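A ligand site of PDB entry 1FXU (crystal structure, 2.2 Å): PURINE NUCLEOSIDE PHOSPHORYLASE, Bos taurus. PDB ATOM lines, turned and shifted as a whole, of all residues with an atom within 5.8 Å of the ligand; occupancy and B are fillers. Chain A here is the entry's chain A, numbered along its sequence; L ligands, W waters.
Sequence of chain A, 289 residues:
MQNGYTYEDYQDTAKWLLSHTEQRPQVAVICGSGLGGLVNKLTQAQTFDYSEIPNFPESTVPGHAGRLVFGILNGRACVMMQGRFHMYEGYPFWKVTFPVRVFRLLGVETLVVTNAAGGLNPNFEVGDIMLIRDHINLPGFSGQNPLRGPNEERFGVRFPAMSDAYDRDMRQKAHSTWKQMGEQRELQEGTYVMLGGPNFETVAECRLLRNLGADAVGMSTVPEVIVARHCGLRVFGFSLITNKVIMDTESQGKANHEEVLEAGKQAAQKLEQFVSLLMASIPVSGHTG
ND2 of Asn 243 lies within hydrogen-bond range of N5 of the ligand.
The side-chain carboxylate (OE1) of Glu 201 is in hydrogen-bond range of a nitrogen (N3) of the ligand.
The side-chain hydroxyl of Thr 242 lies within hydrogen-bond range of a nitrogen (N1) of the ligand.
OH of Tyr 88 is in hydrogen-bond range of O3 of the ligand (2.9 Å).
O2 of the ligand lies within hydrogen-bond range of ND1 of His 257 (3.1 Å).
NE2 of His 86 sits at hydrogen-bond distance from O3 of the ligand (3.5 Å).
N of Gly 119 is in hydrogen-bond range of O of Asn 243 (2.7 Å).
The side-chain carboxylate of Glu 259 sits at hydrogen-bond distance from the side-chain amide nitrogen of Asn 243, 3.5 Å away.
N of Thr 242 is in hydrogen-bond range of O of Ala 117.
O of Gly 118 lies within hydrogen-bond range of N of Val 217 (2.9 Å).
OH of Tyr 192 lies within hydrogen-bond range of N of Met 219, 3.3 Å away.
A ring nitrogen (NE2) of His 64 sits at hydrogen-bond distance from the side-chain hydroxyl (OG) of Ser 33 (2.9 Å).
N of Val 245 sits at hydrogen-bond distance from O of Gly 119, 3.0 Å away.
The backbone carbonyl oxygen (O) of Gly 218 lies within hydrogen-bond range of the backbone NH (N) of Leu 195, 3.1 Å away.
Merely in contact with the ligand: Ser 33 (3.5 Å), Ala 116 (3.4 Å), Ala 117 (3.4 Å), Gly 118 (3.5 Å), Phe 200 (3.5 Å), Val 217 (3.8 Å), Gly 218 (3.7 Å), Met 219 (3.5 Å), Val 245 (3.6 Å) and Val 260 (3.6 Å).
Of the 26 residues printed, 16 come within 4 Å of the ligand.
Water W2 lies within hydrogen-bond range of a nitrogen (N6) of the ligand (2.6 Å) and the backbone carbonyl oxygen (O) of Ala 116 (3.0 Å).
Water W1 lies within hydrogen-bond range of N of Met 219 (2.9 Å) and O3 of the ligand (3.2 Å).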
ATOM      1  N   SER A  33      17.272  20.750  22.367  1.00  0.00           N
ATOM      2  CA  SER A  33      17.261  19.413  21.782  1.00  0.00           C
ATOM      3  C   SER A  33      15.913  18.717  21.984  1.00  0.00           C
ATOM      4  O   SER A  33      15.460  18.526  23.104  1.00  0.00           O
ATOM      5  CB  SER A  33      18.386  18.586  22.423  1.00  0.00           C
ATOM      6  OG  SER A  33      19.676  19.134  22.151  1.00  0.00           O
ATOM      7  N   VAL A  61      24.071  19.943  15.207  1.00  0.00           N
ATOM      8  CA  VAL A  61      23.637  18.865  16.101  1.00  0.00           C
ATOM      9  C   VAL A  61      22.289  18.239  15.744  1.00  0.00           C
ATOM     10  O   VAL A  61      21.320  18.931  15.405  1.00  0.00           O
ATOM     11  CB  VAL A  61      23.541  19.373  17.589  1.00  0.00           C
ATOM     12  CG1 VAL A  61      23.049  18.261  18.506  1.00  0.00           C
ATOM     13  CG2 VAL A  61      24.907  19.889  18.044  1.00  0.00           C
ATOM     14  N   HIS A  64      18.337  19.683  15.891  1.00  0.00           N
ATOM     15  CA  HIS A  64      18.261  21.137  15.750  1.00  0.00           C
ATOM     16  C   HIS A  64      18.101  21.444  14.269  1.00  0.00           C
ATOM     17  O   HIS A  64      19.060  21.376  13.500  1.00  0.00           O
ATOM     18  CB  HIS A  64      19.550  21.800  16.292  1.00  0.00           C
ATOM     19  CG  HIS A  64      19.688  21.729  17.783  1.00  0.00           C
ATOM     20  ND1 HIS A  64      19.590  22.697  18.729  1.00  0.00           N
ATOM     21  CD2 HIS A  64      19.935  20.562  18.463  1.00  0.00           C
ATOM     22  CE1 HIS A  64      19.782  22.085  19.948  1.00  0.00           C
ATOM     23  NE2 HIS A  64      19.989  20.800  19.757  1.00  0.00           N
ATOM     24  N   HIS A  86      25.998  25.357  20.208  1.00  0.00           N
ATOM     25  CA  HIS A  86      26.703  24.917  21.412  1.00  0.00           C
ATOM     26  C   HIS A  86      28.201  25.115  21.247  1.00  0.00           C
ATOM     27  O   HIS A  86      28.767  25.039  20.148  1.00  0.00           O
ATOM     28  CB  HIS A  86      26.431  23.442  21.675  1.00  0.00           C
ATOM     29  CG  HIS A  86      24.993  23.055  21.501  1.00  0.00           C
ATOM     30  ND1 HIS A  86      24.260  22.831  20.388  1.00  0.00           N
ATOM     31  CD2 HIS A  86      24.128  22.867  22.570  1.00  0.00           C
ATOM     32  CE1 HIS A  86      22.990  22.497  20.797  1.00  0.00           C
ATOM     33  NE2 HIS A  86      22.939  22.532  22.113  1.00  0.00           N
ATOM     34  N   TYR A  88      30.524  23.092  22.249  1.00  0.00           N
ATOM     35  CA  TYR A  88      31.198  21.856  21.842  1.00  0.00           C
ATOM     36  C   TYR A  88      31.212  21.663  20.329  1.00  0.00           C
ATOM     37  O   TYR A  88      32.006  20.870  19.802  1.00  0.00           O
ATOM     38  CB  TYR A  88      30.574  20.624  22.525  1.00  0.00           C
ATOM     39  CG  TYR A  88      29.110  20.367  22.197  1.00  0.00           C
ATOM     40  CD1 TYR A  88      28.722  19.969  20.929  1.00  0.00           C
ATOM     41  CD2 TYR A  88      28.132  20.571  23.165  1.00  0.00           C
ATOM     42  CE1 TYR A  88      27.362  19.780  20.614  1.00  0.00           C
ATOM     43  CE2 TYR A  88      26.769  20.388  22.859  1.00  0.00           C
ATOM     44  CZ  TYR A  88      26.401  19.993  21.580  1.00  0.00           C
ATOM     45  OH  TYR A  88      25.050  19.878  21.289  1.00  0.00           O
ATOM     46  N   ALA A 116      17.088  20.513  27.182  1.00  0.00           N
ATOM     47  CA  ALA A 116      16.924  19.161  27.684  1.00  0.00           C
ATOM     48  C   ALA A 116      18.167  19.038  28.581  1.00  0.00           C
ATOM     49  O   ALA A 116      19.240  19.496  28.223  1.00  0.00           O
ATOM     50  CB  ALA A 116      16.981  18.146  26.535  1.00  0.00           C
ATOM     51  N   ALA A 117      18.006  18.451  29.760  1.00  0.00           N
ATOM     52  CA  ALA A 117      19.102  18.358  30.700  1.00  0.00           C
ATOM     53  C   ALA A 117      19.012  17.091  31.525  1.00  0.00           C
ATOM     54  O   ALA A 117      17.973  16.446  31.599  1.00  0.00           O
ATOM     55  CB  ALA A 117      19.065  19.551  31.647  1.00  0.00           C
ATOM     56  N   GLY A 118      20.126  16.772  32.168  1.00  0.00           N
ATOM     57  CA  GLY A 118      20.149  15.601  33.013  1.00  0.00           C
ATOM     58  C   GLY A 118      19.739  16.001  34.403  1.00  0.00           C
ATOM     59  O   GLY A 118      20.122  17.072  34.896  1.00  0.00           O
ATOM     60  N   GLY A 119      18.969  15.138  35.070  1.00  0.00           N
ATOM     61  CA  GLY A 119      18.517  15.418  36.426  1.00  0.00           C
ATOM     62  C   GLY A 119      19.484  14.942  37.491  1.00  0.00           C
ATOM     63  O   GLY A 119      19.830  13.764  37.532  1.00  0.00           O
ATOM     64  N   TYR A 192      20.434  25.316  37.293  1.00  0.00           N
ATOM     65  CA  TYR A 192      20.979  24.628  36.134  1.00  0.00           C
ATOM     66  C   TYR A 192      22.484  24.844  36.084  1.00  0.00           C
ATOM     67  O   TYR A 192      22.980  25.936  36.347  1.00  0.00           O
ATOM     68  CB  TYR A 192      20.294  25.183  34.875  1.00  0.00           C
ATOM     69  CG  TYR A 192      20.839  24.645  33.581  1.00  0.00           C
ATOM     70  CD1 TYR A 192      21.890  25.290  32.928  1.00  0.00           C
ATOM     71  CD2 TYR A 192      20.271  23.527  32.991  1.00  0.00           C
ATOM     72  CE1 TYR A 192      22.357  24.835  31.718  1.00  0.00           C
ATOM     73  CE2 TYR A 192      20.739  23.049  31.772  1.00  0.00           C
ATOM     74  CZ  TYR A 192      21.781  23.712  31.129  1.00  0.00           C
ATOM     75  OH  TYR A 192      22.211  23.298  29.893  1.00  0.00           O
ATOM     76  N   LEU A 195      28.212  22.794  31.609  1.00  0.00           N
ATOM     77  CA  LEU A 195      29.592  22.368  31.395  1.00  0.00           C
ATOM     78  C   LEU A 195      29.790  22.302  29.883  1.00  0.00           C
ATOM     79  O   LEU A 195      28.826  22.436  29.122  1.00  0.00           O
ATOM     80  CB  LEU A 195      29.920  21.038  32.101  1.00  0.00           C
ATOM     81  CG  LEU A 195      28.890  19.934  32.263  1.00  0.00           C
ATOM     82  CD1 LEU A 195      28.404  19.465  30.858  1.00  0.00           C
ATOM     83  CD2 LEU A 195      29.528  18.804  33.072  1.00  0.00           C
ATOM     84  N   PRO A 198      31.441  17.697  24.501  1.00  0.00           N
ATOM     85  CA  PRO A 198      30.223  16.978  24.144  1.00  0.00           C
ATOM     86  C   PRO A 198      30.021  15.620  24.819  1.00  0.00           C
ATOM     87  O   PRO A 198      28.951  15.031  24.679  1.00  0.00           O
ATOM     88  CB  PRO A 198      30.372  16.854  22.638  1.00  0.00           C
ATOM     89  CG  PRO A 198      31.834  16.536  22.516  1.00  0.00           C
ATOM     90  CD  PRO A 198      32.451  17.574  23.431  1.00  0.00           C
ATOM     91  N   ASN A 199      31.032  15.108  25.528  1.00  0.00           N
ATOM     92  CA  ASN A 199      30.860  13.817  26.187  1.00  0.00           C
ATOM     93  C   ASN A 199      29.907  13.988  27.350  1.00  0.00           C
ATOM     94  O   ASN A 199      29.662  15.101  27.799  1.00  0.00           O
ATOM     95  CB  ASN A 199      32.210  13.232  26.691  1.00  0.00           C
ATOM     96  CG  ASN A 199      32.869  14.072  27.774  1.00  0.00           C
ATOM     97  OD1 ASN A 199      32.656  13.864  28.977  1.00  0.00           O
ATOM     98  ND2 ASN A 199      33.678  15.039  27.343  1.00  0.00           N
ATOM     99  N   PHE A 200      29.348  12.864  27.804  1.00  0.00           N
ATOM    100  CA  PHE A 200      28.437  12.844  28.941  1.00  0.00           C
ATOM    101  C   PHE A 200      29.319  12.636  30.168  1.00  0.00           C
ATOM    102  O   PHE A 200      30.407  12.082  30.067  1.00  0.00           O
ATOM    103  CB  PHE A 200      27.400  11.710  28.807  1.00  0.00           C
ATOM    104  CG  PHE A 200      26.255  12.019  27.860  1.00  0.00           C
ATOM    105  CD1 PHE A 200      25.362  13.049  28.138  1.00  0.00           C
ATOM    106  CD2 PHE A 200      26.074  11.270  26.699  1.00  0.00           C
ATOM    107  CE1 PHE A 200      24.283  13.329  27.292  1.00  0.00           C
ATOM    108  CE2 PHE A 200      25.012  11.536  25.841  1.00  0.00           C
ATOM    109  CZ  PHE A 200      24.107  12.573  26.136  1.00  0.00           C
ATOM    110  N   GLU A 201      28.837  13.101  31.317  1.00  0.00           N
ATOM    111  CA  GLU A 201      29.555  13.059  32.584  1.00  0.00           C
ATOM    112  C   GLU A 201      29.870  11.700  33.182  1.00  0.00           C
ATOM    113  O   GLU A 201      29.190  10.727  32.888  1.00  0.00           O
ATOM    114  CB  GLU A 201      28.743  13.850  33.640  1.00  0.00           C
ATOM    115  CG  GLU A 201      28.265  15.220  33.210  1.00  0.00           C
ATOM    116  CD  GLU A 201      27.236  15.171  32.062  1.00  0.00           C
ATOM    117  OE1 GLU A 201      26.299  14.342  32.157  1.00  0.00           O
ATOM    118  OE2 GLU A 201      27.380  15.975  31.085  1.00  0.00           O
ATOM    119  N   VAL A 217      21.851  19.344  34.660  1.00  0.00           N
ATOM    120  CA  VAL A 217      23.067  19.650  33.892  1.00  0.00           C
ATOM    121  C   VAL A 217      22.839  19.675  32.401  1.00  0.00           C
ATOM    122  O   VAL A 217      22.111  18.845  31.851  1.00  0.00           O
ATOM    123  CB  VAL A 217      24.156  18.602  34.131  1.00  0.00           C
ATOM    124  CG1 VAL A 217      24.525  18.572  35.558  1.00  0.00           C
ATOM    125  CG2 VAL A 217      23.634  17.231  33.763  1.00  0.00           C
ATOM    126  N   GLY A 218      23.496  20.600  31.738  1.00  0.00           N
ATOM    127  CA  GLY A 218      23.406  20.703  30.298  1.00  0.00           C
ATOM    128  C   GLY A 218      24.651  21.326  29.707  1.00  0.00           C
ATOM    129  O   GLY A 218      25.606  21.620  30.429  1.00  0.00           O
ATOM    130  N   MET A 219      24.618  21.576  28.401  1.00  0.00           N
ATOM    131  CA  MET A 219      25.759  22.141  27.676  1.00  0.00           C
ATOM    132  C   MET A 219      25.361  23.390  26.900  1.00  0.00           C
ATOM    133  O   MET A 219      25.986  23.718  25.884  1.00  0.00           O
ATOM    134  CB  MET A 219      26.336  21.087  26.707  1.00  0.00           C
ATOM    135  CG  MET A 219      26.783  19.778  27.363  1.00  0.00           C
ATOM    136  SD  MET A 219      26.975  18.385  26.209  1.00  0.00           S
ATOM    137  CE  MET A 219      27.056  17.050  27.366  1.00  0.00           C
ATOM    138  N   THR A 242      15.446  15.005  30.801  1.00  0.00           N
ATOM    139  CA  THR A 242      15.480  13.839  29.935  1.00  0.00           C
ATOM    140  C   THR A 242      16.012  12.565  30.598  1.00  0.00           C
ATOM    141  O   THR A 242      15.876  11.487  30.044  1.00  0.00           O
ATOM    142  CB  THR A 242      16.282  14.118  28.631  1.00  0.00           C
ATOM    143  OG1 THR A 242      17.558  14.673  28.946  1.00  0.00           O
ATOM    144  CG2 THR A 242      15.519  15.097  27.750  1.00  0.00           C
ATOM    145  N   ASN A 243      16.616  12.663  31.772  1.00  0.00           N
ATOM    146  CA  ASN A 243      17.058  11.443  32.412  1.00  0.00           C
ATOM    147  C   ASN A 243      17.638  11.643  33.784  1.00  0.00           C
ATOM    148  O   ASN A 243      18.166  12.712  34.098  1.00  0.00           O
ATOM    149  CB  ASN A 243      18.077  10.683  31.535  1.00  0.00           C
ATOM    150  CG  ASN A 243      19.439  11.325  31.529  1.00  0.00           C
ATOM    151  OD1 ASN A 243      20.200  11.246  32.504  1.00  0.00           O
ATOM    152  ND2 ASN A 243      19.779  11.962  30.419  1.00  0.00           N
ATOM    153  N   VAL A 245      20.420  11.095  36.188  1.00  0.00           N
ATOM    154  CA  VAL A 245      21.830  10.774  36.018  1.00  0.00           C
ATOM    155  C   VAL A 245      22.282   9.709  37.039  1.00  0.00           C
ATOM    156  O   VAL A 245      21.837   9.702  38.190  1.00  0.00           O
ATOM    157  CB  VAL A 245      22.701  12.042  36.140  1.00  0.00           C
ATOM    158  CG1 VAL A 245      24.115  11.751  35.733  1.00  0.00           C
ATOM    159  CG2 VAL A 245      22.140  13.135  35.249  1.00  0.00           C
ATOM    160  N   ALA A 255      24.030   7.350  29.301  1.00  0.00           N
ATOM    161  CA  ALA A 255      23.430   8.416  28.509  1.00  0.00           C
ATOM    162  C   ALA A 255      23.757   8.373  27.025  1.00  0.00           C
ATOM    163  O   ALA A 255      24.865   8.035  26.630  1.00  0.00           O
ATOM    164  CB  ALA A 255      23.830   9.778  29.094  1.00  0.00           C
ATOM    165  N   ASN A 256      22.762   8.717  26.202  1.00  0.00           N
ATOM    166  CA  ASN A 256      22.907   8.743  24.749  1.00  0.00           C
ATOM    167  C   ASN A 256      21.888   9.740  24.198  1.00  0.00           C
ATOM    168  O   ASN A 256      20.744   9.779  24.641  1.00  0.00           O
ATOM    169  CB  ASN A 256      22.672   7.348  24.152  1.00  0.00           C
ATOM    170  CG  ASN A 256      21.358   6.757  24.563  1.00  0.00           C
ATOM    171  OD1 ASN A 256      20.300   7.265  24.187  1.00  0.00           O
ATOM    172  ND2 ASN A 256      21.408   5.689  25.351  1.00  0.00           N
ATOM    173  N   HIS A 257      22.314  10.536  23.233  1.00  0.00           N
ATOM    174  CA  HIS A 257      21.483  11.579  22.642  1.00  0.00           C
ATOM    175  C   HIS A 257      20.104  11.131  22.122  1.00  0.00           C
ATOM    176  O   HIS A 257      19.111  11.833  22.314  1.00  0.00           O
ATOM    177  CB  HIS A 257      22.277  12.290  21.537  1.00  0.00           C
ATOM    178  CG  HIS A 257      21.618  13.518  21.003  1.00  0.00           C
ATOM    179  ND1 HIS A 257      21.295  14.602  21.797  1.00  0.00           N
ATOM    180  CD2 HIS A 257      21.262  13.867  19.736  1.00  0.00           C
ATOM    181  CE1 HIS A 257      20.783  15.561  21.054  1.00  0.00           C
ATOM    182  NE2 HIS A 257      20.751  15.145  19.797  1.00  0.00           N
ATOM    183  N   GLU A 259      18.143   8.880  23.210  1.00  0.00           N
ATOM    184  CA  GLU A 259      17.241   8.777  24.334  1.00  0.00           C
ATOM    185  C   GLU A 259      16.752  10.168  24.772  1.00  0.00           C
ATOM    186  O   GLU A 259      15.587  10.298  25.181  1.00  0.00           O
ATOM    187  CB  GLU A 259      17.933   8.055  25.502  1.00  0.00           C
ATOM    188  CG  GLU A 259      17.598   8.632  26.882  1.00  0.00           C
ATOM    189  CD  GLU A 259      18.634   8.287  27.956  1.00  0.00           C
ATOM    190  OE1 GLU A 259      18.649   7.128  28.435  1.00  0.00           O
ATOM    191  OE2 GLU A 259      19.420   9.191  28.326  1.00  0.00           O
ATOM    192  N   VAL A 260      17.587  11.208  24.687  1.00  0.00           N
ATOM    193  CA  VAL A 260      17.119  12.533  25.103  1.00  0.00           C
ATOM    194  C   VAL A 260      16.095  13.049  24.108  1.00  0.00           C
ATOM    195  O   VAL A 260      15.095  13.653  24.498  1.00  0.00           O
ATOM    196  CB  VAL A 260      18.267  13.605  25.284  1.00  0.00           C
ATOM    197  CG1 VAL A 260      19.542  12.943  25.776  1.00  0.00           C
ATOM    198  CG2 VAL A 260      18.491  14.408  24.012  1.00  0.00           C
HETATM  199  N1  LIG L   1      20.327  15.263  28.938  1.00  0.00           N
HETATM  200  C1  LIG L   1      20.635  16.387  28.207  1.00  0.00           C
HETATM  201  N2  LIG L   1      21.863  16.777  28.443  1.00  0.00           N
HETATM  202  C2  LIG L   1      22.406  15.890  29.343  1.00  0.00           C
HETATM  203  C3  LIG L   1      23.699  15.850  29.974  1.00  0.00           C
HETATM  204  O1  LIG L   1      24.635  16.669  29.836  1.00  0.00           O
HETATM  205  N3  LIG L   1      23.848  14.754  30.857  1.00  0.00           N
HETATM  206  C4  LIG L   1      22.866  13.788  31.068  1.00  0.00           C
HETATM  207  N4  LIG L   1      23.176  12.731  31.872  1.00  0.00           N
HETATM  208  N5  LIG L   1      21.643  13.806  30.444  1.00  0.00           N
HETATM  209  C5  LIG L   1      21.489  14.884  29.611  1.00  0.00           C
HETATM  210  C6  LIG L   1      22.566  17.948  27.901  1.00  0.00           C
HETATM  211  C7  LIG L   1      23.553  17.589  26.821  1.00  0.00           C
HETATM  212  N6  LIG L   1      22.799  17.681  25.571  1.00  0.00           N
HETATM  213  C8  LIG L   1      23.536  17.166  24.407  1.00  0.00           C
HETATM  214  C9  LIG L   1      23.267  15.681  24.223  1.00  0.00           C
HETATM  215  O2  LIG L   1      21.979  15.371  24.673  1.00  0.00           O
HETATM  216  C10 LIG L   1      23.013  17.823  23.138  1.00  0.00           C
HETATM  217  O3  LIG L   1      23.014  19.235  23.261  1.00  0.00           O
HETATM  218  O   HOH W   1      23.152  20.838  25.985  1.00  0.00           O
HETATM  219  O   HOH W   2      20.276  18.274  25.665  1.00  0.00           O
